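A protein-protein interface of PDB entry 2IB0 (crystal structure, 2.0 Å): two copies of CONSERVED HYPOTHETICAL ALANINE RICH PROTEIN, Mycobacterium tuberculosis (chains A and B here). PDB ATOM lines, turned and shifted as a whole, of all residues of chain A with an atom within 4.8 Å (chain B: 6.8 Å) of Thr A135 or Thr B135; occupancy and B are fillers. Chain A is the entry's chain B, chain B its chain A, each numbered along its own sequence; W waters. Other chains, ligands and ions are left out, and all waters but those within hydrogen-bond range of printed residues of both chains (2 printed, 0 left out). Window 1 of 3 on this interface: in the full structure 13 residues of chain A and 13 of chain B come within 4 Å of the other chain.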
ATOM      1  N   SER A 131       3.584  12.023   7.928  1.00  0.00           N
ATOM      2  CA  SER A 131       2.316  11.254   7.876  1.00  0.00           C
ATOM      3  C   SER A 131       1.101  12.128   7.677  1.00  0.00           C
ATOM      4  O   SER A 131       0.228  11.775   6.925  1.00  0.00           O
ATOM      5  CB  SER A 131       2.128  10.311   9.087  1.00  0.00           C
ATOM      6  OG  SER A 131       1.459  10.918  10.201  1.00  0.00           O
ATOM      7  N   THR A 132       1.038  13.259   8.369  1.00  0.00           N
ATOM      8  CA  THR A 132      -0.019  14.238   8.138  1.00  0.00           C
ATOM      9  C   THR A 132      -0.048  14.759   6.704  1.00  0.00           C
ATOM     10  O   THR A 132      -1.105  14.842   6.098  1.00  0.00           O
ATOM     11  CB  THR A 132       0.103  15.396   9.138  1.00  0.00           C
ATOM     12  OG1 THR A 132      -0.052  14.854  10.431  1.00  0.00           O
ATOM     13  CG2 THR A 132      -1.000  16.438   8.943  1.00  0.00           C
ATOM     14  N   ALA A 133       1.110  15.138   6.180  1.00  0.00           N
ATOM     15  CA  ALA A 133       1.238  15.611   4.813  1.00  0.00           C
ATOM     16  C   ALA A 133       0.897  14.523   3.782  1.00  0.00           C
ATOM     17  O   ALA A 133       0.343  14.823   2.729  1.00  0.00           O
ATOM     18  CB  ALA A 133       2.685  16.148   4.570  1.00  0.00           C
ATOM     19  N   LEU A 134       1.277  13.274   4.066  1.00  0.00           N
ATOM     20  CA  LEU A 134       0.960  12.158   3.165  1.00  0.00           C
ATOM     21  C   LEU A 134      -0.546  11.955   3.168  1.00  0.00           C
ATOM     22  O   LEU A 134      -1.173  11.832   2.129  1.00  0.00           O
ATOM     23  CB  LEU A 134       1.710  10.889   3.619  1.00  0.00           C
ATOM     24  CG  LEU A 134       1.261   9.464   3.254  1.00  0.00           C
ATOM     25  CD1 LEU A 134       1.138   9.263   1.768  1.00  0.00           C
ATOM     26  CD2 LEU A 134       2.234   8.443   3.835  1.00  0.00           C
ATOM     27  N   THR A 135      -1.135  11.954   4.349  1.00  0.00           N
ATOM     28  CA  THR A 135      -2.561  11.771   4.456  1.00  0.00           C
ATOM     29  C   THR A 135      -3.381  12.947   3.789  1.00  0.00           C
ATOM     30  O   THR A 135      -4.345  12.688   3.093  1.00  0.00           O
ATOM     31  CB  THR A 135      -2.972  11.493   5.880  1.00  0.00           C
ATOM     32  OG1 THR A 135      -2.414  10.212   6.330  1.00  0.00           O
ATOM     33  CG2 THR A 135      -4.473  11.493   5.970  1.00  0.00           C
ATOM     34  N   GLU A 136      -3.022  14.203   4.036  1.00  0.00           N
ATOM     35  CA  GLU A 136      -3.646  15.345   3.327  1.00  0.00           C
ATOM     36  C   GLU A 136      -3.516  15.226   1.802  1.00  0.00           C
ATOM     37  O   GLU A 136      -4.461  15.581   1.077  1.00  0.00           O
ATOM     38  CB  GLU A 136      -3.072  16.694   3.817  1.00  0.00           C
ATOM     39  CG  GLU A 136      -3.380  16.924   5.344  1.00  0.00           C
ATOM     40  CD  GLU A 136      -2.754  18.211   5.939  1.00  0.00           C
ATOM     41  OE1 GLU A 136      -1.752  18.743   5.428  1.00  0.00           O
ATOM     42  OE2 GLU A 136      -3.247  18.679   6.976  1.00  0.00           O
ATOM     43  N   SER A 137      -2.366  14.723   1.318  1.00  0.00           N
ATOM     44  CA  SER A 137      -2.143  14.568  -0.133  1.00  0.00           C
ATOM     45  C   SER A 137      -3.101  13.552  -0.717  1.00  0.00           C
ATOM     46  O   SER A 137      -3.763  13.828  -1.710  1.00  0.00           O
ATOM     47  CB  SER A 137      -0.690  14.163  -0.461  1.00  0.00           C
ATOM     48  OG  SER A 137       0.224  15.157  -0.043  1.00  0.00           O
ATOM     49  N   ALA A 138      -3.222  12.404  -0.047  1.00  0.00           N
ATOM     50  CA  ALA A 138      -4.120  11.336  -0.436  1.00  0.00           C
ATOM     51  C   ALA A 138      -5.573  11.778  -0.411  1.00  0.00           C
ATOM     52  O   ALA A 138      -6.338  11.419  -1.300  1.00  0.00           O
ATOM     53  CB  ALA A 138      -3.951  10.151   0.489  1.00  0.00           C
ATOM     54  N   VAL A 139      -5.975  12.490   0.648  1.00  0.00           N
ATOM     55  CA  VAL A 139      -7.337  12.985   0.741  1.00  0.00           C
ATOM     56  C   VAL A 139      -7.572  13.992  -0.392  1.00  0.00           C
ATOM     57  O   VAL A 139      -8.619  13.982  -1.045  1.00  0.00           O
ATOM     58  CB  VAL A 139      -7.645  13.601   2.097  1.00  0.00           C
ATOM     59  CG1 VAL A 139      -8.892  14.450   2.001  1.00  0.00           C
ATOM     60  CG2 VAL A 139      -7.848  12.488   3.198  1.00  0.00           C
ATOM     61  N   ARG B  65      -6.465  -5.490   7.047  1.00  0.00           N
ATOM     62  CA  ARG B  65      -5.549  -4.810   7.947  1.00  0.00           C
ATOM     63  C   ARG B  65      -5.386  -5.562   9.277  1.00  0.00           C
ATOM     64  O   ARG B  65      -4.271  -5.772   9.733  1.00  0.00           O
ATOM     65  CB  ARG B  65      -6.066  -3.409   8.229  1.00  0.00           C
ATOM     66  CG  ARG B  65      -5.074  -2.543   8.948  1.00  0.00           C
ATOM     67  CD  ARG B  65      -5.702  -1.216   9.258  1.00  0.00           C
ATOM     68  NE  ARG B  65      -5.982  -0.452   8.058  1.00  0.00           N
ATOM     69  CZ  ARG B  65      -6.961   0.440   7.949  1.00  0.00           C
ATOM     70  NH1 ARG B  65      -7.774   0.663   8.977  1.00  0.00           N
ATOM     71  NH2 ARG B  65      -7.139   1.110   6.807  1.00  0.00           N
ATOM     72  N   ALA B 111      -7.662   6.514  12.622  1.00  0.00           N
ATOM     73  CA  ALA B 111      -6.556   7.448  12.303  1.00  0.00           C
ATOM     74  C   ALA B 111      -5.725   7.773  13.545  1.00  0.00           C
ATOM     75  O   ALA B 111      -4.496   7.683  13.546  1.00  0.00           O
ATOM     76  CB  ALA B 111      -7.089   8.752  11.684  1.00  0.00           C
ATOM     77  N   TRP B 114      -3.638   4.671  14.496  1.00  0.00           N
ATOM     78  CA  TRP B 114      -2.554   4.545  13.526  1.00  0.00           C
ATOM     79  C   TRP B 114      -1.491   5.633  13.567  1.00  0.00           C
ATOM     80  O   TRP B 114      -0.311   5.337  13.380  1.00  0.00           O
ATOM     81  CB  TRP B 114      -3.090   4.294  12.112  1.00  0.00           C
ATOM     82  CG  TRP B 114      -3.706   2.904  12.092  1.00  0.00           C
ATOM     83  CD1 TRP B 114      -5.038   2.597  12.020  1.00  0.00           C
ATOM     84  CD2 TRP B 114      -3.010   1.662  12.209  1.00  0.00           C
ATOM     85  NE1 TRP B 114      -5.218   1.235  12.065  1.00  0.00           N
ATOM     86  CE2 TRP B 114      -3.986   0.634  12.181  1.00  0.00           C
ATOM     87  CE3 TRP B 114      -1.647   1.313  12.326  1.00  0.00           C
ATOM     88  CZ2 TRP B 114      -3.658  -0.710  12.246  1.00  0.00           C
ATOM     89  CZ3 TRP B 114      -1.313  -0.045  12.420  1.00  0.00           C
ATOM     90  CH2 TRP B 114      -2.317  -1.040  12.383  1.00  0.00           C
ATOM     91  N   ARG B 115      -1.877   6.881  13.825  1.00  0.00           N
ATOM     92  CA  ARG B 115      -0.863   7.924  14.030  1.00  0.00           C
ATOM     93  C   ARG B 115       0.035   7.568  15.205  1.00  0.00           C
ATOM     94  O   ARG B 115       1.212   7.860  15.174  1.00  0.00           O
ATOM     95  CB  ARG B 115      -1.510   9.287  14.239  1.00  0.00           C
ATOM     96  CG  ARG B 115      -0.530  10.400  14.357  1.00  0.00           C
ATOM     97  CD  ARG B 115      -1.236  11.760  14.430  1.00  0.00           C
ATOM     98  NE  ARG B 115      -2.228  11.902  13.369  1.00  0.00           N
ATOM     99  CZ  ARG B 115      -3.547  11.892  13.538  1.00  0.00           C
ATOM    100  NH1 ARG B 115      -4.091  11.751  14.756  1.00  0.00           N
ATOM    101  NH2 ARG B 115      -4.332  12.031  12.469  1.00  0.00           N
ATOM    102  N   ALA B 130       1.751   1.557   8.978  1.00  0.00           N
ATOM    103  CA  ALA B 130       0.895   2.320   9.869  1.00  0.00           C
ATOM    104  C   ALA B 130       0.425   3.589   9.131  1.00  0.00           C
ATOM    105  O   ALA B 130      -0.717   3.963   9.257  1.00  0.00           O
ATOM    106  CB  ALA B 130       1.636   2.686  11.159  1.00  0.00           C
ATOM    107  N   SER B 131       1.323   4.240   8.373  1.00  0.00           N
ATOM    108  CA  SER B 131       0.934   5.405   7.633  1.00  0.00           C
ATOM    109  C   SER B 131      -0.052   5.105   6.519  1.00  0.00           C
ATOM    110  O   SER B 131      -0.927   5.921   6.263  1.00  0.00           O
ATOM    111  CB  SER B 131       2.128   6.222   7.123  1.00  0.00           C
ATOM    112  OG  SER B 131       2.635   5.725   5.891  1.00  0.00           O
ATOM    113  N   THR B 132       0.086   3.978   5.843  1.00  0.00           N
ATOM    114  CA  THR B 132      -0.922   3.502   4.894  1.00  0.00           C
ATOM    115  C   THR B 132      -2.314   3.279   5.557  1.00  0.00           C
ATOM    116  O   THR B 132      -3.363   3.781   5.043  1.00  0.00           O
ATOM    117  CB  THR B 132      -0.414   2.233   4.209  1.00  0.00           C
ATOM    118  OG1 THR B 132       0.753   2.585   3.453  1.00  0.00           O
ATOM    119  CG2 THR B 132      -1.462   1.647   3.272  1.00  0.00           C
ATOM    120  N   ALA B 133      -2.309   2.596   6.712  1.00  0.00           N
ATOM    121  CA  ALA B 133      -3.505   2.399   7.526  1.00  0.00           C
ATOM    122  C   ALA B 133      -4.095   3.741   7.984  1.00  0.00           C
ATOM    123  O   ALA B 133      -5.331   3.918   7.964  1.00  0.00           O
ATOM    124  CB  ALA B 133      -3.193   1.499   8.712  1.00  0.00           C
ATOM    125  N   LEU B 134      -3.232   4.689   8.362  1.00  0.00           N
ATOM    126  CA  LEU B 134      -3.691   5.989   8.796  1.00  0.00           C
ATOM    127  C   LEU B 134      -4.389   6.745   7.627  1.00  0.00           C
ATOM    128  O   LEU B 134      -5.475   7.328   7.781  1.00  0.00           O
ATOM    129  CB  LEU B 134      -2.488   6.805   9.282  1.00  0.00           C
ATOM    130  CG  LEU B 134      -2.580   8.069  10.151  1.00  0.00           C
ATOM    131  CD1 LEU B 134      -1.318   8.823  10.036  1.00  0.00           C
ATOM    132  CD2 LEU B 134      -3.704   8.977   9.830  1.00  0.00           C
ATOM    133  N   THR B 135      -3.722   6.741   6.479  1.00  0.00           N
ATOM    134  CA  THR B 135      -4.237   7.395   5.273  1.00  0.00           C
ATOM    135  C   THR B 135      -5.554   6.777   4.793  1.00  0.00           C
ATOM    136  O   THR B 135      -6.485   7.522   4.429  1.00  0.00           O
ATOM    137  CB  THR B 135      -3.210   7.339   4.177  1.00  0.00           C
ATOM    138  OG1 THR B 135      -2.089   8.162   4.559  1.00  0.00           O
ATOM    139  CG2 THR B 135      -3.789   7.825   2.849  1.00  0.00           C
ATOM    140  N   GLU B 136      -5.638   5.449   4.810  1.00  0.00           N
ATOM    141  CA  GLU B 136      -6.878   4.753   4.447  1.00  0.00           C
ATOM    142  C   GLU B 136      -8.074   5.101   5.351  1.00  0.00           C
ATOM    143  O   GLU B 136      -9.193   5.227   4.834  1.00  0.00           O
ATOM    144  CB  GLU B 136      -6.685   3.238   4.402  1.00  0.00           C
ATOM    145  CG  GLU B 136      -5.759   2.834   3.229  1.00  0.00           C
ATOM    146  CD  GLU B 136      -5.404   1.359   3.240  1.00  0.00           C
ATOM    147  OE1 GLU B 136      -5.643   0.657   4.250  1.00  0.00           O
ATOM    148  OE2 GLU B 136      -4.881   0.880   2.223  1.00  0.00           O
ATOM    149  N   SER B 137      -7.813   5.190   6.666  1.00  0.00           N
ATOM    150  CA  SER B 137      -8.783   5.557   7.704  1.00  0.00           C
ATOM    151  C   SER B 137      -9.292   6.981   7.419  1.00  0.00           C
ATOM    152  O   SER B 137     -10.480   7.242   7.444  1.00  0.00           O
ATOM    153  CB  SER B 137      -8.113   5.525   9.094  1.00  0.00           C
ATOM    154  OG  SER B 137      -7.725   4.220   9.491  1.00  0.00           O
ATOM    155  N   ALA B 138      -8.368   7.898   7.167  1.00  0.00           N
ATOM    156  CA  ALA B 138      -8.687   9.279   6.735  1.00  0.00           C
ATOM    157  C   ALA B 138      -9.476   9.402   5.433  1.00  0.00           C
ATOM    158  O   ALA B 138     -10.357  10.232   5.331  1.00  0.00           O
ATOM    159  CB  ALA B 138      -7.428  10.054   6.597  1.00  0.00           C
ATOM    160  N   VAL B 139      -9.104   8.650   4.405  1.00  0.00           N
ATOM    161  CA  VAL B 139      -9.847   8.639   3.147  1.00  0.00           C
ATOM    162  C   VAL B 139     -11.247   8.028   3.429  1.00  0.00           C
ATOM    163  O   VAL B 139     -12.285   8.581   3.001  1.00  0.00           O
ATOM    164  CB  VAL B 139      -9.056   7.897   2.069  1.00  0.00           C
ATOM    165  CG1 VAL B 139      -9.946   7.520   0.902  1.00  0.00           C
ATOM    166  CG2 VAL B 139      -7.818   8.778   1.593  1.00  0.00           C
ATOM    167  N   MET B 140     -11.311   6.956   4.223  1.00  0.00           N
ATOM    168  CA  MET B 140     -12.636   6.385   4.577  1.00  0.00           C
ATOM    169  C   MET B 140     -13.572   7.374   5.273  1.00  0.00           C
ATOM    170  O   MET B 140     -14.767   7.443   4.930  1.00  0.00           O
ATOM    171  CB  MET B 140     -12.531   5.104   5.415  1.00  0.00           C
ATOM    172  CG  MET B 140     -12.371   3.788   4.622  1.00  0.00           C
ATOM    173  SD  MET B 140     -13.614   3.415   3.322  1.00  0.00           S
ATOM    174  CE  MET B 140     -14.972   4.050   4.061  1.00  0.00           C
HETATM  175  O   HOH W   1       0.165   8.658   6.816  1.00  0.00           O
HETATM  176  O   HOH W   2      -0.724  12.379  11.012  1.00  0.00           O
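OG1 of Thr B135 lies within hydrogen-bond range of OG1 of Thr A135, 2.7 Å away.
The backbone carbonyl oxygen of Ser B131 sits at hydrogen-bond distance from the side-chain hydroxyl of Thr B135 (3.0 Å). The backbone carbonyl oxygen (O) of Ser A131 is in hydrogen-bond range of the side-chain hydroxyl (OG1) of Thr A135 (3.1 Å).
Among the printed residues, pairs that only touch across the chains: Ala A138 with Thr B135 (3.3 Å), Thr A135 with Ala B138 (3.3 Å), Leu A134 with Ser B131 (3.4 Å), Ser A131 with Leu B134 (3.5 Å), Leu A134 with Thr B135 (3.8 Å), Thr A135 with Leu B134 (3.9 Å) and Val A139 with Ala B138 (3.99 Å).
Of the printed residues of chain B, Thr A135 touches Leu B134, Thr B135 and Ala B138. Of chain A, only Leu A134 (3.8 Å), Thr A135 (2.7 Å) and Ala A138 (3.3 Å) come within 4 Å of Thr B135. Of the printed residues of chain A, Ala B138 touches Thr A135 and Val A139. Of the printed residues of chain A, Ser B131 touches Leu A134. The nearest residue of chain B that does not touch Thr A135 is Ser B131 (4.5 Å). The nearest printed residue of chain A that does not touch Thr B135 is Ser A131 (4.9 Å). The nearest printed residue of chain A that does not touch Ser B131 is Ser A131 (4.5 Å).
Hydrophobic or aromatic side chains of chain A that line the printed part of chain B: Leu A134, Ala A138 and Val A139. Of the 15 printed residues of chain B, 4 touch a printed residue of chain A. Among the printed residues, 8 pairs touch across the chains. Among the printed residues, no Asp or Glu carboxylate lies within 4 Å of a Lys or Arg side-chain nitrogen of the other chain.
Ser A131 touches Leu B134, and with the chains exchanged Leu A134 touches Ser B131. Leu A134 touches Thr B135, and with the chains exchanged Thr A135 touches Leu B134. Thr A135 touches its own counterpart, Thr B135. Val A139 touches Ala B138, but with the chains exchanged Ala A138 does not touch Val B139 (4.2 Å). 9 positions are printed for both chains. Of the 8 pairs that touch across the chains among the printed residues, 7 have their exchanged pair printed and touching as well.
Water W2 lies within hydrogen-bond range of OG1 of Thr A132, OG of Ser A131 and NE of Arg B115. Water W1 lies within hydrogen-bond range of O of Ser B131, OG1 of Thr A135, O of Ser A131 and OG1 of Thr B135.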
